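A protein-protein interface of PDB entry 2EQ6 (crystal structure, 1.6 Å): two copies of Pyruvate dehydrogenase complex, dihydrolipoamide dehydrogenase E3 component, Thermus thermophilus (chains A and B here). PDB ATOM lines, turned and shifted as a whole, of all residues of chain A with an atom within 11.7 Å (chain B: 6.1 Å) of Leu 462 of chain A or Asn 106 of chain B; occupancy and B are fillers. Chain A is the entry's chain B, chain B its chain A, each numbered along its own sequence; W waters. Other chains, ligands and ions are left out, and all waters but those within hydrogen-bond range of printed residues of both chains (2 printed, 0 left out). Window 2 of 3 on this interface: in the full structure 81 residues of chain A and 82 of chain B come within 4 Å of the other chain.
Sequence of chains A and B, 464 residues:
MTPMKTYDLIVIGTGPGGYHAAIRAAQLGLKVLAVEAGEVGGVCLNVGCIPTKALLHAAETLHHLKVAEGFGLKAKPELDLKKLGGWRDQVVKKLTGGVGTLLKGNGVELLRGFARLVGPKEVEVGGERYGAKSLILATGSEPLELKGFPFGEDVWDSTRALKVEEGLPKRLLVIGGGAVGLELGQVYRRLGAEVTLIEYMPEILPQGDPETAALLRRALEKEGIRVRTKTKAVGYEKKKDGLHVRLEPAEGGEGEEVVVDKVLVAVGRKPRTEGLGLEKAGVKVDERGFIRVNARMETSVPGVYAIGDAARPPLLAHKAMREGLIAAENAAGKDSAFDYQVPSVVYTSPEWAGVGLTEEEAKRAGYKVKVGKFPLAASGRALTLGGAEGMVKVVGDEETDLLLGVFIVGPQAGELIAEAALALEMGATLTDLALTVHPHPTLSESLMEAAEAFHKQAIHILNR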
ATOM      1  N   VAL A 371      34.636  -0.621 -18.902  1.00  0.00           N
ATOM      2  CA  VAL A 371      34.480  -1.688 -17.923  1.00  0.00           C
ATOM      3  C   VAL A 371      33.483  -2.760 -18.326  1.00  0.00           C
ATOM      4  O   VAL A 371      32.605  -2.533 -19.162  1.00  0.00           O
ATOM      5  CB  VAL A 371      34.040  -1.133 -16.554  1.00  0.00           C
ATOM      6  CG1 VAL A 371      34.994  -0.044 -16.107  1.00  0.00           C
ATOM      7  CG2 VAL A 371      32.615  -0.607 -16.632  1.00  0.00           C
ATOM      8  N   GLY A 372      33.642  -3.931 -17.716  1.00  0.00           N
ATOM      9  CA  GLY A 372      32.756  -5.049 -17.959  1.00  0.00           C
ATOM     10  C   GLY A 372      32.337  -5.565 -16.598  1.00  0.00           C
ATOM     11  O   GLY A 372      33.172  -5.678 -15.698  1.00  0.00           O
ATOM     12  N   LYS A 373      31.054  -5.862 -16.428  1.00  0.00           N
ATOM     13  CA  LYS A 373      30.557  -6.351 -15.148  1.00  0.00           C
ATOM     14  C   LYS A 373      29.738  -7.622 -15.293  1.00  0.00           C
ATOM     15  O   LYS A 373      29.037  -7.811 -16.286  1.00  0.00           O
ATOM     16  CB  LYS A 373      29.656  -5.309 -14.482  1.00  0.00           C
ATOM     17  CG  LYS A 373      30.240  -3.923 -14.325  1.00  0.00           C
ATOM     18  CD  LYS A 373      29.205  -3.016 -13.663  1.00  0.00           C
ATOM     19  CE  LYS A 373      29.669  -1.571 -13.579  1.00  0.00           C
ATOM     20  NZ  LYS A 373      28.651  -0.730 -12.881  1.00  0.00           N
ATOM     21  N   PHE A 374      29.828  -8.492 -14.291  1.00  0.00           N
ATOM     22  CA  PHE A 374      29.037  -9.716 -14.274  1.00  0.00           C
ATOM     23  C   PHE A 374      28.582  -9.928 -12.838  1.00  0.00           C
ATOM     24  O   PHE A 374      29.405 -10.081 -11.937  1.00  0.00           O
ATOM     25  CB  PHE A 374      29.834 -10.941 -14.730  1.00  0.00           C
ATOM     26  CG  PHE A 374      28.983 -12.176 -14.882  1.00  0.00           C
ATOM     27  CD1 PHE A 374      28.088 -12.288 -15.945  1.00  0.00           C
ATOM     28  CD2 PHE A 374      29.019 -13.190 -13.928  1.00  0.00           C
ATOM     29  CE1 PHE A 374      27.238 -13.391 -16.057  1.00  0.00           C
ATOM     30  CE2 PHE A 374      28.170 -14.303 -14.028  1.00  0.00           C
ATOM     31  CZ  PHE A 374      27.278 -14.399 -15.097  1.00  0.00           C
ATOM     32  N   PRO A 375      27.261  -9.922 -12.604  1.00  0.00           N
ATOM     33  CA  PRO A 375      26.688 -10.112 -11.269  1.00  0.00           C
ATOM     34  C   PRO A 375      26.592 -11.591 -10.917  1.00  0.00           C
ATOM     35  O   PRO A 375      26.248 -12.406 -11.770  1.00  0.00           O
ATOM     36  CB  PRO A 375      25.318  -9.471 -11.403  1.00  0.00           C
ATOM     37  CG  PRO A 375      24.929  -9.877 -12.792  1.00  0.00           C
ATOM     38  CD  PRO A 375      26.201  -9.672 -13.600  1.00  0.00           C
ATOM     39  N   ALA A 377      24.449 -12.866  -9.342  1.00  0.00           N
ATOM     40  CA  ALA A 377      23.036 -13.211  -9.367  1.00  0.00           C
ATOM     41  C   ALA A 377      22.772 -14.036 -10.627  1.00  0.00           C
ATOM     42  O   ALA A 377      21.792 -14.773 -10.698  1.00  0.00           O
ATOM     43  CB  ALA A 377      22.187 -11.945  -9.377  1.00  0.00           C
ATOM     44  N   ALA A 378      23.658 -13.910 -11.612  1.00  0.00           N
ATOM     45  CA  ALA A 378      23.528 -14.643 -12.869  1.00  0.00           C
ATOM     46  C   ALA A 378      24.438 -15.870 -12.913  1.00  0.00           C
ATOM     47  O   ALA A 378      24.575 -16.509 -13.958  1.00  0.00           O
ATOM     48  CB  ALA A 378      23.846 -13.720 -14.044  1.00  0.00           C
ATOM     49  N   SER A 379      25.062 -16.192 -11.785  1.00  0.00           N
ATOM     50  CA  SER A 379      25.960 -17.343 -11.706  1.00  0.00           C
ATOM     51  C   SER A 379      25.255 -18.601 -11.211  1.00  0.00           C
ATOM     52  O   SER A 379      24.717 -18.625 -10.107  1.00  0.00           O
ATOM     53  CB  SER A 379      27.136 -17.035 -10.772  1.00  0.00           C
ATOM     54  OG  SER A 379      27.879 -18.213 -10.482  1.00  0.00           O
ATOM     55  N   GLU A 449      33.018 -14.117 -18.158  1.00  0.00           N
ATOM     56  CA  GLU A 449      31.791 -13.433 -18.559  1.00  0.00           C
ATOM     57  C   GLU A 449      31.888 -11.917 -18.424  1.00  0.00           C
ATOM     58  O   GLU A 449      31.284 -11.183 -19.202  1.00  0.00           O
ATOM     59  CB  GLU A 449      30.601 -13.967 -17.760  1.00  0.00           C
ATOM     60  CG  GLU A 449      30.372 -15.459 -17.964  1.00  0.00           C
ATOM     61  CD  GLU A 449      28.905 -15.825 -18.008  1.00  0.00           C
ATOM     62  OE1 GLU A 449      28.173 -15.238 -18.836  1.00  0.00           O
ATOM     63  OE2 GLU A 449      28.484 -16.701 -17.220  1.00  0.00           O
ATOM     64  N   ALA A 450      32.648 -11.445 -17.442  1.00  0.00           N
ATOM     65  CA  ALA A 450      32.811 -10.006 -17.271  1.00  0.00           C
ATOM     66  C   ALA A 450      33.588  -9.465 -18.471  1.00  0.00           C
ATOM     67  O   ALA A 450      33.345  -8.346 -18.927  1.00  0.00           O
ATOM     68  CB  ALA A 450      33.551  -9.708 -15.972  1.00  0.00           C
ATOM     69  N   GLU A 452      33.458 -10.783 -21.444  1.00  0.00           N
ATOM     70  CA  GLU A 452      32.505 -10.810 -22.548  1.00  0.00           C
ATOM     71  C   GLU A 452      31.606  -9.577 -22.463  1.00  0.00           C
ATOM     72  O   GLU A 452      31.254  -8.981 -23.483  1.00  0.00           O
ATOM     73  CB  GLU A 452      31.651 -12.082 -22.483  1.00  0.00           C
ATOM     74  CG  GLU A 452      32.393 -13.350 -22.871  1.00  0.00           C
ATOM     75  CD  GLU A 452      32.398 -13.591 -24.370  1.00  0.00           C
ATOM     76  OE1 GLU A 452      32.752 -12.662 -25.125  1.00  0.00           O
ATOM     77  OE2 GLU A 452      32.045 -14.712 -24.796  1.00  0.00           O
ATOM     78  N   ALA A 453      31.241  -9.195 -21.242  1.00  0.00           N
ATOM     79  CA  ALA A 453      30.384  -8.032 -21.024  1.00  0.00           C
ATOM     80  C   ALA A 453      31.112  -6.757 -21.447  1.00  0.00           C
ATOM     81  O   ALA A 453      30.493  -5.806 -21.924  1.00  0.00           O
ATOM     82  CB  ALA A 453      29.974  -7.949 -19.556  1.00  0.00           C
ATOM     83  N   PHE A 454      32.427  -6.748 -21.263  1.00  0.00           N
ATOM     84  CA  PHE A 454      33.257  -5.610 -21.645  1.00  0.00           C
ATOM     85  C   PHE A 454      33.114  -5.407 -23.156  1.00  0.00           C
ATOM     86  O   PHE A 454      33.080  -4.276 -23.640  1.00  0.00           O
ATOM     87  CB  PHE A 454      34.716  -5.897 -21.248  1.00  0.00           C
ATOM     88  CG  PHE A 454      35.713  -4.884 -21.745  1.00  0.00           C
ATOM     89  CD1 PHE A 454      36.214  -4.957 -23.040  1.00  0.00           C
ATOM     90  CD2 PHE A 454      36.185  -3.880 -20.901  1.00  0.00           C
ATOM     91  CE1 PHE A 454      37.170  -4.049 -23.489  1.00  0.00           C
ATOM     92  CE2 PHE A 454      37.144  -2.966 -21.342  1.00  0.00           C
ATOM     93  CZ  PHE A 454      37.636  -3.052 -22.637  1.00  0.00           C
ATOM     94  N   HIS A 455      33.003  -6.514 -23.887  1.00  0.00           N
ATOM     95  CA  HIS A 455      32.853  -6.486 -25.341  1.00  0.00           C
ATOM     96  C   HIS A 455      31.377  -6.482 -25.758  1.00  0.00           C
ATOM     97  O   HIS A 455      31.051  -6.675 -26.933  1.00  0.00           O
ATOM     98  CB  HIS A 455      33.560  -7.696 -25.959  1.00  0.00           C
ATOM     99  CG  HIS A 455      35.051  -7.664 -25.820  1.00  0.00           C
ATOM    100  ND1 HIS A 455      35.811  -8.806 -25.692  1.00  0.00           N
ATOM    101  CD2 HIS A 455      35.927  -6.631 -25.826  1.00  0.00           C
ATOM    102  CE1 HIS A 455      37.089  -8.480 -25.624  1.00  0.00           C
ATOM    103  NE2 HIS A 455      37.186  -7.165 -25.704  1.00  0.00           N
ATOM    104  N   LYS A 456      30.495  -6.272 -24.784  1.00  0.00           N
ATOM    105  CA  LYS A 456      29.053  -6.214 -25.019  1.00  0.00           C
ATOM    106  C   LYS A 456      28.433  -7.493 -25.583  1.00  0.00           C
ATOM    107  O   LYS A 456      27.418  -7.435 -26.281  1.00  0.00           O
ATOM    108  CB  LYS A 456      28.727  -5.042 -25.954  1.00  0.00           C
ATOM    109  CG  LYS A 456      29.227  -3.695 -25.458  1.00  0.00           C
ATOM    110  CD  LYS A 456      28.535  -3.278 -24.172  1.00  0.00           C
ATOM    111  CE  LYS A 456      29.026  -1.914 -23.709  1.00  0.00           C
ATOM    112  NZ  LYS A 456      28.334  -1.453 -22.473  1.00  0.00           N
ATOM    113  N   GLN A 457      29.026  -8.644 -25.289  1.00  0.00           N
ATOM    114  CA  GLN A 457      28.472  -9.898 -25.789  1.00  0.00           C
ATOM    115  C   GLN A 457      28.390 -11.011 -24.752  1.00  0.00           C
ATOM    116  O   GLN A 457      28.539 -12.190 -25.080  1.00  0.00           O
ATOM    117  CB  GLN A 457      29.250 -10.383 -27.018  1.00  0.00           C
ATOM    118  CG  GLN A 457      30.755 -10.464 -26.849  1.00  0.00           C
ATOM    119  CD  GLN A 457      31.432 -11.062 -28.070  1.00  0.00           C
ATOM    120  OE1 GLN A 457      31.039 -10.790 -29.205  1.00  0.00           O
ATOM    121  NE2 GLN A 457      32.460 -11.870 -27.843  1.00  0.00           N
ATOM    122  N   ALA A 458      28.148 -10.638 -23.500  1.00  0.00           N
ATOM    123  CA  ALA A 458      28.006 -11.625 -22.436  1.00  0.00           C
ATOM    124  C   ALA A 458      26.765 -12.445 -22.772  1.00  0.00           C
ATOM    125  O   ALA A 458      25.807 -11.919 -23.336  1.00  0.00           O
ATOM    126  CB  ALA A 458      27.827 -10.932 -21.093  1.00  0.00           C
ATOM    127  N   ILE A 459      26.775 -13.726 -22.422  1.00  0.00           N
ATOM    128  CA  ILE A 459      25.644 -14.599 -22.719  1.00  0.00           C
ATOM    129  C   ILE A 459      24.575 -14.690 -21.632  1.00  0.00           C
ATOM    130  O   ILE A 459      23.381 -14.630 -21.928  1.00  0.00           O
ATOM    131  CB  ILE A 459      26.129 -16.036 -23.030  1.00  0.00           C
ATOM    132  CG1 ILE A 459      27.049 -16.027 -24.251  1.00  0.00           C
ATOM    133  CG2 ILE A 459      24.933 -16.952 -23.262  1.00  0.00           C
ATOM    134  CD1 ILE A 459      26.384 -15.565 -25.536  1.00  0.00           C
ATOM    135  N   HIS A 460      25.004 -14.829 -20.380  1.00  0.00           N
ATOM    136  CA  HIS A 460      24.085 -14.982 -19.253  1.00  0.00           C
ATOM    137  C   HIS A 460      23.425 -13.723 -18.696  1.00  0.00           C
ATOM    138  O   HIS A 460      22.727 -13.773 -17.684  1.00  0.00           O
ATOM    139  CB  HIS A 460      24.790 -15.758 -18.140  1.00  0.00           C
ATOM    140  CG  HIS A 460      25.042 -17.193 -18.490  1.00  0.00           C
ATOM    141  ND1 HIS A 460      26.190 -17.862 -18.123  1.00  0.00           N
ATOM    142  CD2 HIS A 460      24.287 -18.088 -19.172  1.00  0.00           C
ATOM    143  CE1 HIS A 460      26.132 -19.107 -18.563  1.00  0.00           C
ATOM    144  NE2 HIS A 460      24.987 -19.269 -19.203  1.00  0.00           N
ATOM    145  N   ILE A 461      23.650 -12.597 -19.358  1.00  0.00           N
ATOM    146  CA  ILE A 461      23.030 -11.339 -18.965  1.00  0.00           C
ATOM    147  C   ILE A 461      22.805 -10.539 -20.234  1.00  0.00           C
ATOM    148  O   ILE A 461      23.545 -10.688 -21.208  1.00  0.00           O
ATOM    149  CB  ILE A 461      23.912 -10.498 -18.005  1.00  0.00           C
ATOM    150  CG1 ILE A 461      25.293 -10.270 -18.619  1.00  0.00           C
ATOM    151  CG2 ILE A 461      24.005 -11.178 -16.649  1.00  0.00           C
ATOM    152  CD1 ILE A 461      26.152  -9.297 -17.837  1.00  0.00           C
ATOM    153  N   LEU A 462      21.769  -9.710 -20.236  1.00  0.00           N
ATOM    154  CA  LEU A 462      21.484  -8.882 -21.398  1.00  0.00           C
ATOM    155  C   LEU A 462      22.543  -7.784 -21.439  1.00  0.00           C
ATOM    156  O   LEU A 462      22.939  -7.256 -20.398  1.00  0.00           O
ATOM    157  CB  LEU A 462      20.084  -8.275 -21.285  1.00  0.00           C
ATOM    158  CG  LEU A 462      18.933  -9.284 -21.207  1.00  0.00           C
ATOM    159  CD1 LEU A 462      17.622  -8.546 -20.989  1.00  0.00           C
ATOM    160  CD2 LEU A 462      18.877 -10.115 -22.484  1.00  0.00           C
ATOM    161  N   ASN A 463      23.009  -7.456 -22.638  1.00  0.00           N
ATOM    162  CA  ASN A 463      24.032  -6.433 -22.817  1.00  0.00           C
ATOM    163  C   ASN A 463      23.410  -5.091 -23.187  1.00  0.00           C
ATOM    164  O   ASN A 463      23.673  -4.105 -22.469  1.00  0.00           O
ATOM    165  CB  ASN A 463      25.015  -6.869 -23.908  1.00  0.00           C
ATOM    166  CG  ASN A 463      25.763  -8.140 -23.545  1.00  0.00           C
ATOM    167  OD1 ASN A 463      26.723  -8.113 -22.772  1.00  0.00           O
ATOM    168  ND2 ASN A 463      25.316  -9.264 -24.091  1.00  0.00           N
ATOM    169  N   ALA B  22      22.306 -19.906 -29.908  1.00  0.00           N
ATOM    170  CA  ALA B  22      21.127 -19.089 -30.209  1.00  0.00           C
ATOM    171  C   ALA B  22      21.322 -17.634 -29.800  1.00  0.00           C
ATOM    172  O   ALA B  22      21.018 -16.714 -30.563  1.00  0.00           O
ATOM    173  CB  ALA B  22      19.895 -19.657 -29.514  1.00  0.00           C
ATOM    174  N   ILE B  23      21.824 -17.423 -28.591  1.00  0.00           N
ATOM    175  CA  ILE B  23      22.036 -16.063 -28.118  1.00  0.00           C
ATOM    176  C   ILE B  23      23.146 -15.320 -28.858  1.00  0.00           C
ATOM    177  O   ILE B  23      22.968 -14.161 -29.230  1.00  0.00           O
ATOM    178  CB  ILE B  23      22.305 -16.057 -26.605  1.00  0.00           C
ATOM    179  CG1 ILE B  23      21.015 -16.446 -25.874  1.00  0.00           C
ATOM    180  CG2 ILE B  23      22.795 -14.679 -26.154  1.00  0.00           C
ATOM    181  CD1 ILE B  23      21.152 -16.576 -24.376  1.00  0.00           C
ATOM    182  N   ALA B  26      21.930 -14.297 -32.170  1.00  0.00           N
ATOM    183  CA  ALA B  26      20.991 -13.182 -32.073  1.00  0.00           C
ATOM    184  C   ALA B  26      21.755 -11.872 -31.880  1.00  0.00           C
ATOM    185  O   ALA B  26      21.405 -10.846 -32.468  1.00  0.00           O
ATOM    186  CB  ALA B  26      20.017 -13.408 -30.915  1.00  0.00           C
ATOM    187  N   GLN B  27      22.804 -11.913 -31.062  1.00  0.00           N
ATOM    188  CA  GLN B  27      23.613 -10.725 -30.805  1.00  0.00           C
ATOM    189  C   GLN B  27      24.254 -10.240 -32.097  1.00  0.00           C
ATOM    190  O   GLN B  27      24.498  -9.044 -32.270  1.00  0.00           O
ATOM    191  CB  GLN B  27      24.720 -11.033 -29.795  1.00  0.00           C
ATOM    192  CG  GLN B  27      24.242 -11.499 -28.435  1.00  0.00           C
ATOM    193  CD  GLN B  27      25.400 -11.883 -27.538  1.00  0.00           C
ATOM    194  OE1 GLN B  27      26.435 -12.342 -28.018  1.00  0.00           O
ATOM    195  NE2 GLN B  27      25.229 -11.711 -26.232  1.00  0.00           N
ATOM    196  N   LEU B  30      21.231 -12.191 -36.336  1.00  0.00           N
ATOM    197  CA  LEU B  30      20.497 -13.228 -37.053  1.00  0.00           C
ATOM    198  C   LEU B  30      19.116 -13.479 -36.463  1.00  0.00           C
ATOM    199  O   LEU B  30      18.886 -13.271 -35.269  1.00  0.00           O
ATOM    200  CB  LEU B  30      21.285 -14.544 -37.061  1.00  0.00           C
ATOM    201  CG  LEU B  30      22.538 -14.642 -37.936  1.00  0.00           C
ATOM    202  CD1 LEU B  30      23.104 -16.054 -37.858  1.00  0.00           C
ATOM    203  CD2 LEU B  30      22.193 -14.304 -39.381  1.00  0.00           C
ATOM    204  N   THR B 101      14.205 -16.613 -20.212  1.00  0.00           N
ATOM    205  CA  THR B 101      14.117 -15.157 -20.214  1.00  0.00           C
ATOM    206  C   THR B 101      15.197 -14.543 -21.103  1.00  0.00           C
ATOM    207  O   THR B 101      14.961 -13.542 -21.781  1.00  0.00           O
ATOM    208  CB  THR B 101      14.251 -14.600 -18.778  1.00  0.00           C
ATOM    209  OG1 THR B 101      13.149 -15.062 -17.987  1.00  0.00           O
ATOM    210  CG2 THR B 101      14.263 -13.080 -18.785  1.00  0.00           C
ATOM    211  N   LEU B 102      16.380 -15.149 -21.104  1.00  0.00           N
ATOM    212  CA  LEU B 102      17.483 -14.664 -21.926  1.00  0.00           C
ATOM    213  C   LEU B 102      17.193 -14.862 -23.410  1.00  0.00           C
ATOM    214  O   LEU B 102      17.501 -14.001 -24.232  1.00  0.00           O
ATOM    215  CB  LEU B 102      18.781 -15.388 -21.559  1.00  0.00           C
ATOM    216  CG  LEU B 102      19.424 -15.039 -20.214  1.00  0.00           C
ATOM    217  CD1 LEU B 102      20.566 -16.003 -19.930  1.00  0.00           C
ATOM    218  CD2 LEU B 102      19.929 -13.605 -20.241  1.00  0.00           C
ATOM    219  N   LEU B 103      16.609 -16.005 -23.757  1.00  0.00           N
ATOM    220  CA  LEU B 103      16.287 -16.286 -25.148  1.00  0.00           C
ATOM    221  C   LEU B 103      15.282 -15.252 -25.648  1.00  0.00           C
ATOM    222  O   LEU B 103      15.452 -14.675 -26.719  1.00  0.00           O
ATOM    223  CB  LEU B 103      15.706 -17.699 -25.286  1.00  0.00           C
ATOM    224  CG  LEU B 103      16.699 -18.844 -25.041  1.00  0.00           C
ATOM    225  CD1 LEU B 103      15.968 -20.179 -25.028  1.00  0.00           C
ATOM    226  CD2 LEU B 103      17.766 -18.830 -26.121  1.00  0.00           C
ATOM    227  N   LYS B 104      14.244 -15.018 -24.856  1.00  0.00           N
ATOM    228  CA  LYS B 104      13.209 -14.053 -25.209  1.00  0.00           C
ATOM    229  C   LYS B 104      13.804 -12.649 -25.281  1.00  0.00           C
ATOM    230  O   LYS B 104      13.543 -11.902 -26.224  1.00  0.00           O
ATOM    231  CB  LYS B 104      12.084 -14.096 -24.173  1.00  0.00           C
ATOM    232  CG  LYS B 104      10.956 -13.109 -24.418  1.00  0.00           C
ATOM    233  CD  LYS B 104       9.888 -13.236 -23.342  1.00  0.00           C
ATOM    234  CE  LYS B 104       8.792 -12.195 -23.517  1.00  0.00           C
ATOM    235  NZ  LYS B 104       8.109 -12.319 -24.836  1.00  0.00           N
ATOM    236  N   GLY B 105      14.617 -12.306 -24.285  1.00  0.00           N
ATOM    237  CA  GLY B 105      15.241 -10.996 -24.252  1.00  0.00           C
ATOM    238  C   GLY B 105      16.147 -10.735 -25.441  1.00  0.00           C
ATOM    239  O   GLY B 105      16.376  -9.582 -25.811  1.00  0.00           O
ATOM    240  N   ASN B 106      16.666 -11.802 -26.041  1.00  0.00           N
ATOM    241  CA  ASN B 106      17.551 -11.680 -27.194  1.00  0.00           C
ATOM    242  C   ASN B 106      16.809 -11.797 -28.523  1.00  0.00           C
ATOM    243  O   ASN B 106      17.421 -11.747 -29.591  1.00  0.00           O
ATOM    244  CB  ASN B 106      18.659 -12.736 -27.120  1.00  0.00           C
ATOM    245  CG  ASN B 106      19.829 -12.285 -26.269  1.00  0.00           C
ATOM    246  OD1 ASN B 106      20.699 -11.552 -26.735  1.00  0.00           O
ATOM    247  ND2 ASN B 106      19.849 -12.707 -25.010  1.00  0.00           N
ATOM    248  N   GLY B 107      15.492 -11.956 -28.452  1.00  0.00           N
ATOM    249  CA  GLY B 107      14.696 -12.059 -29.660  1.00  0.00           C
ATOM    250  C   GLY B 107      14.715 -13.422 -30.327  1.00  0.00           C
ATOM    251  O   GLY B 107      14.378 -13.543 -31.503  1.00  0.00           O
ATOM    252  N   VAL B 108      15.114 -14.449 -29.584  1.00  0.00           N
ATOM    253  CA  VAL B 108      15.151 -15.802 -30.125  1.00  0.00           C
ATOM    254  C   VAL B 108      13.773 -16.440 -29.973  1.00  0.00           C
ATOM    255  O   VAL B 108      13.192 -16.421 -28.892  1.00  0.00           O
ATOM    256  CB  VAL B 108      16.187 -16.680 -29.380  1.00  0.00           C
ATOM    257  CG1 VAL B 108      16.122 -18.113 -29.899  1.00  0.00           C
ATOM    258  CG2 VAL B 108      17.585 -16.109 -29.565  1.00  0.00           C
HETATM  259  O   HOH W   1      22.231 -12.453 -23.099  1.00  0.00           O
HETATM  260  O   HOH W   2      22.717 -10.673 -25.456  1.00  0.00           O
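The side-chain amide nitrogen (NE2) of Gln 27 of chain B sits close to the side-chain amide nitrogen (ND2) of Asn 463 of chain A, at 3.3 Å.
The side-chain amide nitrogen of Gln 27 of chain B is in hydrogen-bond range of the backbone carbonyl oxygen of Ala 458 of chain A (3.0 Å).
A ring nitrogen (ND1) of His 460 of chain A lies within hydrogen-bond range of the side-chain carboxylate (OE2) of Glu 449 of chain A (2.7 Å).
The backbone NH (N) of Gln 457 of chain A lies within hydrogen-bond range of the side-chain amide oxygen (OD1) of Asn 463 of chain A.
O of Ala 458 of chain A sits at hydrogen-bond distance from ND2 of Asn 463 of chain A (2.8 Å).
O of Leu 102 of chain B sits at hydrogen-bond distance from ND2 of Asn 106 of chain B (2.8 Å).
The side-chain amide nitrogen of Gln 457 of chain A is in hydrogen-bond range of the side-chain carboxylate of Glu 452 of chain A (2.8 Å).
Among the printed residues, merely in contact across the chains: Gln 457 of chain A with Gln 27 of chain B, Ile 459 of chain A with Ile 23 of chain B, Ile 459 of chain A with Leu 102 of chain B, His 460 of chain A with Leu 102 of chain B, Ile 461 of chain A with Leu 102 of chain B and Leu 462 of chain A with Asn 106 of chain B.
Of the printed residues of chain B, Gln 457 of chain A touches Gln 27.
Printed residues of chain B within 4 Å of Ala 458 of chain A: Gln 27 (3.0 Å).
Of the printed residues of chain B, Ile 461 of chain A touches Leu 102.
Leu 462 of chain A touches just one residue of chain B: Asn 106.
Printed residues of chain B within 4 Å of Asn 463 of chain A: Gln 27 (3.3 Å).
Of chain A, only Gln 457 (3.5 Å), Ala 458 (3.0 Å) and Asn 463 (3.3 Å) come within 4 Å of Gln 27 of chain B.
Leu 102 of chain B touches just these residues of chain A: Ile 459, His 460 and Ile 461.
No residue of chain A comes within 4 Å of Gly 105 of chain B.
Of chain A, only Leu 462 comes within 4 Å of Asn 106 of chain B.
No residue of chain A comes within 4 Å of Gly 107 of chain B.
The nearest residue of chain A that does not touch Asn 106 of chain B is Ile 459 of chain A (5.1 Å).
Of the 22 printed residues of chain A, 7 touch a printed residue of chain B.
Printed residues of chain A that touch a printed residue of chain B: Gln 457, Ala 458, Ile 459, His 460, Ile 461, Leu 462 and Asn 463.
Among the printed residues, 8 pairs touch across the chains.
No position is printed for both chains.
Of the 8 pairs that touch across the chains among the printed residues, none has its exchanged pair printed and touching as well.
Water W2 lies within hydrogen-bond range of OD1 of Asn 106 of chain B, NE2 of Gln 27 of chain B and ND2 of Asn 463 of chain A.
Water W1 lies within hydrogen-bond range of O of Ile 459 of chain A, O of Ile 461 of chain A and ND2 of Asn 106 of chain B.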
